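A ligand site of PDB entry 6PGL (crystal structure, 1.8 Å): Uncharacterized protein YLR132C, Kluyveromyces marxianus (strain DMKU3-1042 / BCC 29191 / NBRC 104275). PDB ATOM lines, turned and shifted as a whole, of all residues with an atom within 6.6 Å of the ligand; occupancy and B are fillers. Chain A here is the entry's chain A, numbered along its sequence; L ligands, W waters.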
ATOM      1  N   PHE A  11      24.013 -22.749 -27.101  1.00  0.00           N
ATOM      2  CA  PHE A  11      22.821 -22.024 -26.645  1.00  0.00           C
ATOM      3  C   PHE A  11      21.623 -22.907 -26.972  1.00  0.00           C
ATOM      4  O   PHE A  11      21.555 -23.438 -28.081  1.00  0.00           O
ATOM      5  CB  PHE A  11      22.745 -20.644 -27.340  1.00  0.00           C
ATOM      6  CG  PHE A  11      21.404 -19.976 -27.244  1.00  0.00           C
ATOM      7  CD1 PHE A  11      20.521 -20.031 -28.311  1.00  0.00           C
ATOM      8  CD2 PHE A  11      21.025 -19.304 -26.097  1.00  0.00           C
ATOM      9  CE1 PHE A  11      19.267 -19.428 -28.246  1.00  0.00           C
ATOM     10  CE2 PHE A  11      19.756 -18.674 -26.018  1.00  0.00           C
ATOM     11  CZ  PHE A  11      18.881 -18.743 -27.101  1.00  0.00           C
ATOM     12  N   LEU A  48       9.482  -9.775 -35.540  1.00  0.00           N
ATOM     13  CA  LEU A  48      10.498 -10.815 -35.553  1.00  0.00           C
ATOM     14  C   LEU A  48      10.093 -12.043 -36.343  1.00  0.00           C
ATOM     15  O   LEU A  48      10.965 -12.882 -36.633  1.00  0.00           O
ATOM     16  CB  LEU A  48      10.857 -11.233 -34.118  1.00  0.00           C
ATOM     17  CG  LEU A  48      11.683 -10.146 -33.387  1.00  0.00           C
ATOM     18  CD1 LEU A  48      11.743 -10.394 -31.897  1.00  0.00           C
ATOM     19  CD2 LEU A  48      13.097 -10.152 -33.980  1.00  0.00           C
ATOM     20  N   HIS A  60      11.297 -17.849 -30.953  1.00  0.00           N
ATOM     21  CA  HIS A  60      11.989 -18.799 -30.097  1.00  0.00           C
ATOM     22  C   HIS A  60      11.701 -18.538 -28.624  1.00  0.00           C
ATOM     23  O   HIS A  60      11.260 -17.451 -28.243  1.00  0.00           O
ATOM     24  CB  HIS A  60      13.529 -18.782 -30.332  1.00  0.00           C
ATOM     25  CG  HIS A  60      14.204 -17.506 -29.943  1.00  0.00           C
ATOM     26  ND1 HIS A  60      14.334 -16.436 -30.805  1.00  0.00           N
ATOM     27  CD2 HIS A  60      14.800 -17.112 -28.784  1.00  0.00           C
ATOM     28  CE1 HIS A  60      14.965 -15.447 -30.203  1.00  0.00           C
ATOM     29  NE2 HIS A  60      15.259 -15.836 -28.971  1.00  0.00           N
ATOM     30  N   VAL A  61      11.866 -19.590 -27.824  1.00  0.00           N
ATOM     31  CA  VAL A  61      12.008 -19.485 -26.377  1.00  0.00           C
ATOM     32  C   VAL A  61      13.465 -19.795 -26.069  1.00  0.00           C
ATOM     33  O   VAL A  61      13.908 -20.929 -26.265  1.00  0.00           O
ATOM     34  CB  VAL A  61      11.055 -20.436 -25.611  1.00  0.00           C
ATOM     35  CG1 VAL A  61      11.149 -20.191 -24.064  1.00  0.00           C
ATOM     36  CG2 VAL A  61       9.626 -20.294 -26.091  1.00  0.00           C
ATOM     37  N   SER A  62      14.216 -18.816 -25.567  1.00  0.00           N
ATOM     38  CA  SER A  62      15.556 -19.095 -25.066  1.00  0.00           C
ATOM     39  C   SER A  62      15.460 -19.989 -23.849  1.00  0.00           C
ATOM     40  O   SER A  62      14.584 -19.799 -22.983  1.00  0.00           O
ATOM     41  CB  SER A  62      16.305 -17.815 -24.691  1.00  0.00           C
ATOM     42  OG  SER A  62      16.434 -16.919 -25.786  1.00  0.00           O
ATOM     43  N   LEU A  63      16.324 -21.007 -23.784  1.00  0.00           N
ATOM     44  CA  LEU A  63      16.354 -21.915 -22.655  1.00  0.00           C
ATOM     45  C   LEU A  63      17.675 -21.906 -21.896  1.00  0.00           C
ATOM     46  O   LEU A  63      17.798 -22.636 -20.913  1.00  0.00           O
ATOM     47  CB  LEU A  63      16.021 -23.347 -23.106  1.00  0.00           C
ATOM     48  CG  LEU A  63      14.636 -23.570 -23.742  1.00  0.00           C
ATOM     49  CD1 LEU A  63      14.541 -24.997 -24.314  1.00  0.00           C
ATOM     50  CD2 LEU A  63      13.467 -23.282 -22.780  1.00  0.00           C
ATOM     51  N   VAL A 104       8.939  -5.436 -22.018  1.00  0.00           N
ATOM     52  CA  VAL A 104      10.029  -4.938 -22.869  1.00  0.00           C
ATOM     53  C   VAL A 104      11.351  -5.275 -22.203  1.00  0.00           C
ATOM     54  O   VAL A 104      11.636  -4.802 -21.090  1.00  0.00           O
ATOM     55  CB  VAL A 104       9.923  -3.434 -23.174  1.00  0.00           C
ATOM     56  CG1 VAL A 104      10.965  -3.002 -24.231  1.00  0.00           C
ATOM     57  CG2 VAL A 104       8.540  -3.085 -23.645  1.00  0.00           C
ATOM     58  N   TYR A 105      12.153  -6.088 -22.877  1.00  0.00           N
ATOM     59  CA  TYR A 105      13.485  -6.487 -22.415  1.00  0.00           C
ATOM     60  C   TYR A 105      14.531  -5.707 -23.198  1.00  0.00           C
ATOM     61  O   TYR A 105      14.430  -5.563 -24.423  1.00  0.00           O
ATOM     62  CB  TYR A 105      13.704  -7.982 -22.639  1.00  0.00           C
ATOM     63  CG  TYR A 105      12.966  -8.915 -21.713  1.00  0.00           C
ATOM     64  CD1 TYR A 105      13.417  -9.147 -20.413  1.00  0.00           C
ATOM     65  CD2 TYR A 105      11.842  -9.642 -22.151  1.00  0.00           C
ATOM     66  CE1 TYR A 105      12.753 -10.035 -19.544  1.00  0.00           C
ATOM     67  CE2 TYR A 105      11.164 -10.530 -21.284  1.00  0.00           C
ATOM     68  CZ  TYR A 105      11.646 -10.714 -19.984  1.00  0.00           C
ATOM     69  OH  TYR A 105      11.025 -11.581 -19.111  1.00  0.00           O
ATOM     70  N   GLU A 106      15.557  -5.216 -22.493  1.00  0.00           N
ATOM     71  CA  GLU A 106      16.729  -4.606 -23.108  1.00  0.00           C
ATOM     72  C   GLU A 106      17.807  -5.650 -23.259  1.00  0.00           C
ATOM     73  O   GLU A 106      17.987  -6.484 -22.378  1.00  0.00           O
ATOM     74  CB  GLU A 106      17.290  -3.481 -22.239  1.00  0.00           C
ATOM     75  CG  GLU A 106      16.668  -2.173 -22.456  1.00  0.00           C
ATOM     76  CD  GLU A 106      17.586  -1.030 -22.120  1.00  0.00           C
ATOM     77  OE1 GLU A 106      18.438  -1.172 -21.224  1.00  0.00           O
ATOM     78  OE2 GLU A 106      17.428   0.040 -22.751  1.00  0.00           O
ATOM     79  N   ASN A 107      18.551  -5.597 -24.380  1.00  0.00           N
ATOM     80  CA  ASN A 107      19.659  -6.517 -24.547  1.00  0.00           C
ATOM     81  C   ASN A 107      20.882  -5.987 -23.802  1.00  0.00           C
ATOM     82  O   ASN A 107      20.847  -4.907 -23.204  1.00  0.00           O
ATOM     83  CB  ASN A 107      19.934  -6.786 -26.033  1.00  0.00           C
ATOM     84  CG  ASN A 107      20.511  -5.571 -26.755  1.00  0.00           C
ATOM     85  OD1 ASN A 107      20.343  -4.427 -26.313  1.00  0.00           O
ATOM     86  ND2 ASN A 107      21.168  -5.816 -27.879  1.00  0.00           N
ATOM     87  N   PHE A 108      21.976  -6.729 -23.895  1.00  0.00           N
ATOM     88  CA  PHE A 108      23.115  -6.560 -22.990  1.00  0.00           C
ATOM     89  C   PHE A 108      23.764  -5.191 -23.118  1.00  0.00           C
ATOM     90  O   PHE A 108      24.311  -4.669 -22.132  1.00  0.00           O
ATOM     91  CB  PHE A 108      24.162  -7.650 -23.252  1.00  0.00           C
ATOM     92  CG  PHE A 108      25.054  -7.347 -24.418  1.00  0.00           C
ATOM     93  CD1 PHE A 108      24.571  -7.467 -25.727  1.00  0.00           C
ATOM     94  CD2 PHE A 108      26.360  -6.914 -24.228  1.00  0.00           C
ATOM     95  CE1 PHE A 108      25.380  -7.187 -26.809  1.00  0.00           C
ATOM     96  CE2 PHE A 108      27.191  -6.648 -25.323  1.00  0.00           C
ATOM     97  CZ  PHE A 108      26.697  -6.769 -26.604  1.00  0.00           C
ATOM     98  N   LEU A 112      19.044  -2.657 -28.121  1.00  0.00           N
ATOM     99  CA  LEU A 112      17.779  -3.164 -28.651  1.00  0.00           C
ATOM    100  C   LEU A 112      16.775  -3.376 -27.523  1.00  0.00           C
ATOM    101  O   LEU A 112      17.140  -3.777 -26.404  1.00  0.00           O
ATOM    102  CB  LEU A 112      17.966  -4.476 -29.411  1.00  0.00           C
ATOM    103  CG  LEU A 112      18.940  -4.405 -30.592  1.00  0.00           C
ATOM    104  CD1 LEU A 112      19.115  -5.788 -31.185  1.00  0.00           C
ATOM    105  CD2 LEU A 112      18.376  -3.409 -31.638  1.00  0.00           C
ATOM    106  N   PHE A 114      13.211  -5.403 -26.803  1.00  0.00           N
ATOM    107  CA  PHE A 114      12.407  -6.500 -27.332  1.00  0.00           C
ATOM    108  C   PHE A 114      11.015  -6.440 -26.717  1.00  0.00           C
ATOM    109  O   PHE A 114      10.883  -6.406 -25.493  1.00  0.00           O
ATOM    110  CB  PHE A 114      13.081  -7.844 -27.036  1.00  0.00           C
ATOM    111  CG  PHE A 114      14.293  -8.111 -27.882  1.00  0.00           C
ATOM    112  CD1 PHE A 114      15.540  -7.616 -27.499  1.00  0.00           C
ATOM    113  CD2 PHE A 114      14.195  -8.849 -29.063  1.00  0.00           C
ATOM    114  CE1 PHE A 114      16.688  -7.876 -28.284  1.00  0.00           C
ATOM    115  CE2 PHE A 114      15.312  -9.106 -29.835  1.00  0.00           C
ATOM    116  CZ  PHE A 114      16.559  -8.611 -29.451  1.00  0.00           C
ATOM    117  N   ALA A 116       7.817  -8.374 -25.757  1.00  0.00           N
ATOM    118  CA  ALA A 116       7.673  -9.798 -25.467  1.00  0.00           C
ATOM    119  C   ALA A 116       6.474 -10.048 -24.554  1.00  0.00           C
ATOM    120  O   ALA A 116       5.905  -9.134 -23.932  1.00  0.00           O
ATOM    121  CB  ALA A 116       8.943 -10.338 -24.822  1.00  0.00           C
ATOM    122  N   GLN A 146      22.948 -11.921 -18.286  1.00  0.00           N
ATOM    123  CA  GLN A 146      21.549 -12.275 -18.010  1.00  0.00           C
ATOM    124  C   GLN A 146      21.353 -13.787 -18.065  1.00  0.00           C
ATOM    125  O   GLN A 146      21.331 -14.365 -19.159  1.00  0.00           O
ATOM    126  CB  GLN A 146      20.603 -11.580 -18.991  1.00  0.00           C
ATOM    127  N   PRO A 147      21.201 -14.466 -16.928  1.00  0.00           N
ATOM    128  CA  PRO A 147      20.884 -15.898 -16.957  1.00  0.00           C
ATOM    129  C   PRO A 147      19.431 -16.122 -17.351  1.00  0.00           C
ATOM    130  O   PRO A 147      18.577 -15.242 -17.230  1.00  0.00           O
ATOM    131  CB  PRO A 147      21.132 -16.346 -15.517  1.00  0.00           C
ATOM    132  CG  PRO A 147      20.772 -15.131 -14.720  1.00  0.00           C
ATOM    133  CD  PRO A 147      21.169 -13.924 -15.552  1.00  0.00           C
ATOM    134  N   VAL A 148      19.168 -17.330 -17.861  1.00  0.00           N
ATOM    135  CA  VAL A 148      17.855 -17.720 -18.353  1.00  0.00           C
ATOM    136  C   VAL A 148      17.293 -18.745 -17.392  1.00  0.00           C
ATOM    137  O   VAL A 148      17.953 -19.742 -17.068  1.00  0.00           O
ATOM    138  CB  VAL A 148      17.927 -18.296 -19.780  1.00  0.00           C
ATOM    139  CG1 VAL A 148      16.603 -18.969 -20.143  1.00  0.00           C
ATOM    140  CG2 VAL A 148      18.277 -17.191 -20.780  1.00  0.00           C
ATOM    141  N   ASN A 151      12.026 -17.703 -14.204  1.00  0.00           N
ATOM    142  CA  ASN A 151      11.461 -16.406 -13.877  1.00  0.00           C
ATOM    143  C   ASN A 151      11.394 -15.463 -15.083  1.00  0.00           C
ATOM    144  O   ASN A 151      10.688 -14.459 -15.004  1.00  0.00           O
ATOM    145  CB  ASN A 151      12.309 -15.744 -12.786  1.00  0.00           C
ATOM    146  CG  ASN A 151      13.747 -15.446 -13.270  1.00  0.00           C
ATOM    147  OD1 ASN A 151      14.056 -14.331 -13.686  1.00  0.00           O
ATOM    148  ND2 ASN A 151      14.595 -16.469 -13.247  1.00  0.00           N
ATOM    149  N   ASN A 152      12.081 -15.779 -16.192  1.00  0.00           N
ATOM    150  CA  ASN A 152      12.103 -14.863 -17.332  1.00  0.00           C
ATOM    151  C   ASN A 152      11.843 -15.560 -18.671  1.00  0.00           C
ATOM    152  O   ASN A 152      12.162 -15.000 -19.713  1.00  0.00           O
ATOM    153  CB  ASN A 152      13.419 -14.076 -17.392  1.00  0.00           C
ATOM    154  CG  ASN A 152      14.649 -14.975 -17.557  1.00  0.00           C
ATOM    155  OD1 ASN A 152      14.571 -16.092 -18.078  1.00  0.00           O
ATOM    156  ND2 ASN A 152      15.810 -14.483 -17.114  1.00  0.00           N
ATOM    157  N   HIS A 154      10.125 -16.353 -21.936  1.00  0.00           N
ATOM    158  CA  HIS A 154       9.276 -15.462 -22.702  1.00  0.00           C
ATOM    159  C   HIS A 154       9.480 -15.734 -24.192  1.00  0.00           C
ATOM    160  O   HIS A 154      10.433 -16.404 -24.594  1.00  0.00           O
ATOM    161  CB  HIS A 154       9.613 -14.004 -22.381  1.00  0.00           C
ATOM    162  CG  HIS A 154      10.965 -13.616 -22.881  1.00  0.00           C
ATOM    163  ND1 HIS A 154      12.115 -13.832 -22.164  1.00  0.00           N
ATOM    164  CD2 HIS A 154      11.351 -13.082 -24.071  1.00  0.00           C
ATOM    165  CE1 HIS A 154      13.166 -13.446 -22.872  1.00  0.00           C
ATOM    166  NE2 HIS A 154      12.731 -12.982 -24.040  1.00  0.00           N
ATOM    167  N   VAL A 155       8.581 -15.190 -24.999  1.00  0.00           N
ATOM    168  CA  VAL A 155       8.742 -15.113 -26.448  1.00  0.00           C
ATOM    169  C   VAL A 155       8.794 -13.644 -26.829  1.00  0.00           C
ATOM    170  O   VAL A 155       7.900 -12.876 -26.455  1.00  0.00           O
ATOM    171  CB  VAL A 155       7.574 -15.807 -27.192  1.00  0.00           C
ATOM    172  CG1 VAL A 155       7.721 -15.593 -28.699  1.00  0.00           C
ATOM    173  CG2 VAL A 155       7.504 -17.323 -26.857  1.00  0.00           C
ATOM    174  N   SER A 156       9.834 -13.233 -27.558  1.00  0.00           N
ATOM    175  CA  SER A 156       9.876 -11.890 -28.130  1.00  0.00           C
ATOM    176  C   SER A 156       9.186 -11.856 -29.482  1.00  0.00           C
ATOM    177  O   SER A 156       9.370 -12.751 -30.318  1.00  0.00           O
ATOM    178  CB  SER A 156      11.311 -11.400 -28.295  1.00  0.00           C
ATOM    179  OG  SER A 156      11.894 -11.219 -27.018  1.00  0.00           O
ATOM    180  N   ARG A 180       7.514   0.970 -21.730  1.00  0.00           N
ATOM    181  CA  ARG A 180       6.816  -0.171 -21.134  1.00  0.00           C
ATOM    182  C   ARG A 180       5.397   0.180 -20.741  1.00  0.00           C
ATOM    183  O   ARG A 180       4.458  -0.588 -20.983  1.00  0.00           O
ATOM    184  CB  ARG A 180       7.562  -0.680 -19.912  1.00  0.00           C
ATOM    185  CG  ARG A 180       8.807  -1.467 -20.257  1.00  0.00           C
ATOM    186  CD  ARG A 180       9.758  -1.459 -19.073  1.00  0.00           C
ATOM    187  NE  ARG A 180      10.790  -2.446 -19.291  1.00  0.00           N
ATOM    188  CZ  ARG A 180      11.915  -2.502 -18.588  1.00  0.00           C
ATOM    189  NH1 ARG A 180      12.152  -1.606 -17.634  1.00  0.00           N
ATOM    190  NH2 ARG A 180      12.812  -3.460 -18.844  1.00  0.00           N
HETATM  191  N1  LIG L   1      16.693 -10.439 -21.302  1.00  0.00           N
HETATM  192  C1  LIG L   1      16.618  -9.501 -20.244  1.00  0.00           C
HETATM  193  N2  LIG L   1      16.152  -9.882 -19.041  1.00  0.00           N
HETATM  194  C2  LIG L   1      15.763 -11.135 -18.829  1.00  0.00           C
HETATM  195  C3  LIG L   1      15.841 -12.076 -19.857  1.00  0.00           C
HETATM  196  C4  LIG L   1      16.326 -11.707 -21.103  1.00  0.00           C
HETATM  197  O1  LIG L   1      16.966  -8.298 -20.382  1.00  0.00           O
HETATM  198  O2  LIG L   1      15.333 -11.428 -17.703  1.00  0.00           O
HETATM  199  C5  LIG L   1      17.218 -10.028 -22.616  1.00  0.00           C
HETATM  200  C6  LIG L   1      18.215 -11.012 -23.207  1.00  0.00           C
HETATM  201  O3  LIG L   1      19.502 -10.783 -22.695  1.00  0.00           O
HETATM  202  C7  LIG L   1      18.092 -10.748 -24.706  1.00  0.00           C
HETATM  203  C8  LIG L   1      16.665 -10.198 -24.870  1.00  0.00           C
HETATM  204  O4  LIG L   1      19.032  -9.752 -25.080  1.00  0.00           O
HETATM  205  O5  LIG L   1      16.159  -9.953 -23.540  1.00  0.00           O
HETATM  206  C9  LIG L   1      15.707 -11.105 -25.613  1.00  0.00           C
HETATM  207  O6  LIG L   1      15.997 -12.483 -25.404  1.00  0.00           O
HETATM  208  P1  LIG L   1      15.227 -13.624 -26.206  1.00  0.00           P
HETATM  209  O7  LIG L   1      15.321 -14.816 -25.306  1.00  0.00           O
HETATM  210  O8  LIG L   1      13.811 -13.114 -26.418  1.00  0.00           O
HETATM  211  O9  LIG L   1      16.054 -13.801 -27.452  1.00  0.00           O
HETATM  212  O   HOH W   1      16.480 -14.493 -22.658  1.00  0.00           O
HETATM  213  O   HOH W   2      20.284  -8.738 -21.231  1.00  0.00           O
HETATM  214  O   HOH W   3      13.090 -16.292 -24.983  1.00  0.00           O
HETATM  215  O   HOH W   4      12.725 -10.929 -16.364  1.00  0.00           O
HETATM  216  O   HOH W   5      22.200 -10.632 -21.757  1.00  0.00           O
HETATM  217  O   HOH W   6      15.743  -5.805 -19.616  1.00  0.00           O
HETATM  218  O   HOH W   7      12.130 -14.828 -28.021  1.00  0.00           O
HETATM  219  O   HOH W   8      21.768  -9.574 -24.792  1.00  0.00           O
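An oxygen (O7) of the ligand sits at hydrogen-bond distance from the side-chain hydroxyl (OG) of Ser 62, at 2.4 Å.
A ring nitrogen (NE2) of His 154 lies within hydrogen-bond range of an oxygen (O8) of the ligand (2.6 Å).
A ring nitrogen (NE2) of His 60 lies within hydrogen-bond range of an oxygen (O9) of the ligand (2.7 Å).
The side-chain hydroxyl (OG) of Ser 156 is in hydrogen-bond range of an oxygen (O8) of the ligand, 2.8 Å away.
ND2 of Asn 152 is in hydrogen-bond range of O2 of the ligand (3.1 Å).
A ring nitrogen (ND1) of His 154 is in hydrogen-bond range of the backbone carbonyl oxygen (O) of Asn 152 (2.7 Å).
O of Tyr 105 sits at hydrogen-bond distance from N of Phe 114 (2.7 Å).
The side-chain amide nitrogen of Asn 152 lies within hydrogen-bond range of the backbone carbonyl oxygen of Pro 147 (2.9 Å).
The backbone NH of Leu 112 sits at hydrogen-bond distance from the side-chain amide oxygen of Asn 107 (2.8 Å).
An oxygen (O1) of the ligand sits close to the backbone carbonyl oxygen (O) of Glu 106, 2.9 Å away.
Merely in contact with the ligand: Tyr 105 (3.1 Å), Asn 107 (3.2 Å), Phe 114 (3.9 Å) and Gln 146 (3.9 Å).
Hydrophobic or aromatic side chains within 4 Å of the ligand: His 60, Tyr 105, Phe 114 and His 154.
Within 4 Å of the ligand: His 60, Ser 62, Tyr 105, Glu 106, Asn 107, Phe 114, Gln 146, Asn 152, His 154 and Ser 156.
Water W2 lies within hydrogen-bond range of O3 of the ligand (2.6 Å) and O of Glu 106 (3.4 Å).
Water W3 lies within hydrogen-bond range of the backbone carbonyl oxygen (O) of His 154, an oxygen (O7) of the ligand and the backbone NH (N) of Ser 62.
Water W8 lies within hydrogen-bond range of O4 of the ligand and N of Phe 108.
Water W6 bridges an oxygen (O1) of the ligand (2.9 Å) and the backbone NH (N) of Glu 106 (2.9 Å).
Water W7 lies within hydrogen-bond range of O of His 60 (2.8 Å), N of Ser 156 (2.8 Å) and O8 of the ligand (2.9 Å).
Water W4 lies within hydrogen-bond range of O2 of the ligand (3.0 Å) and OH of Tyr 105 (3.3 Å).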
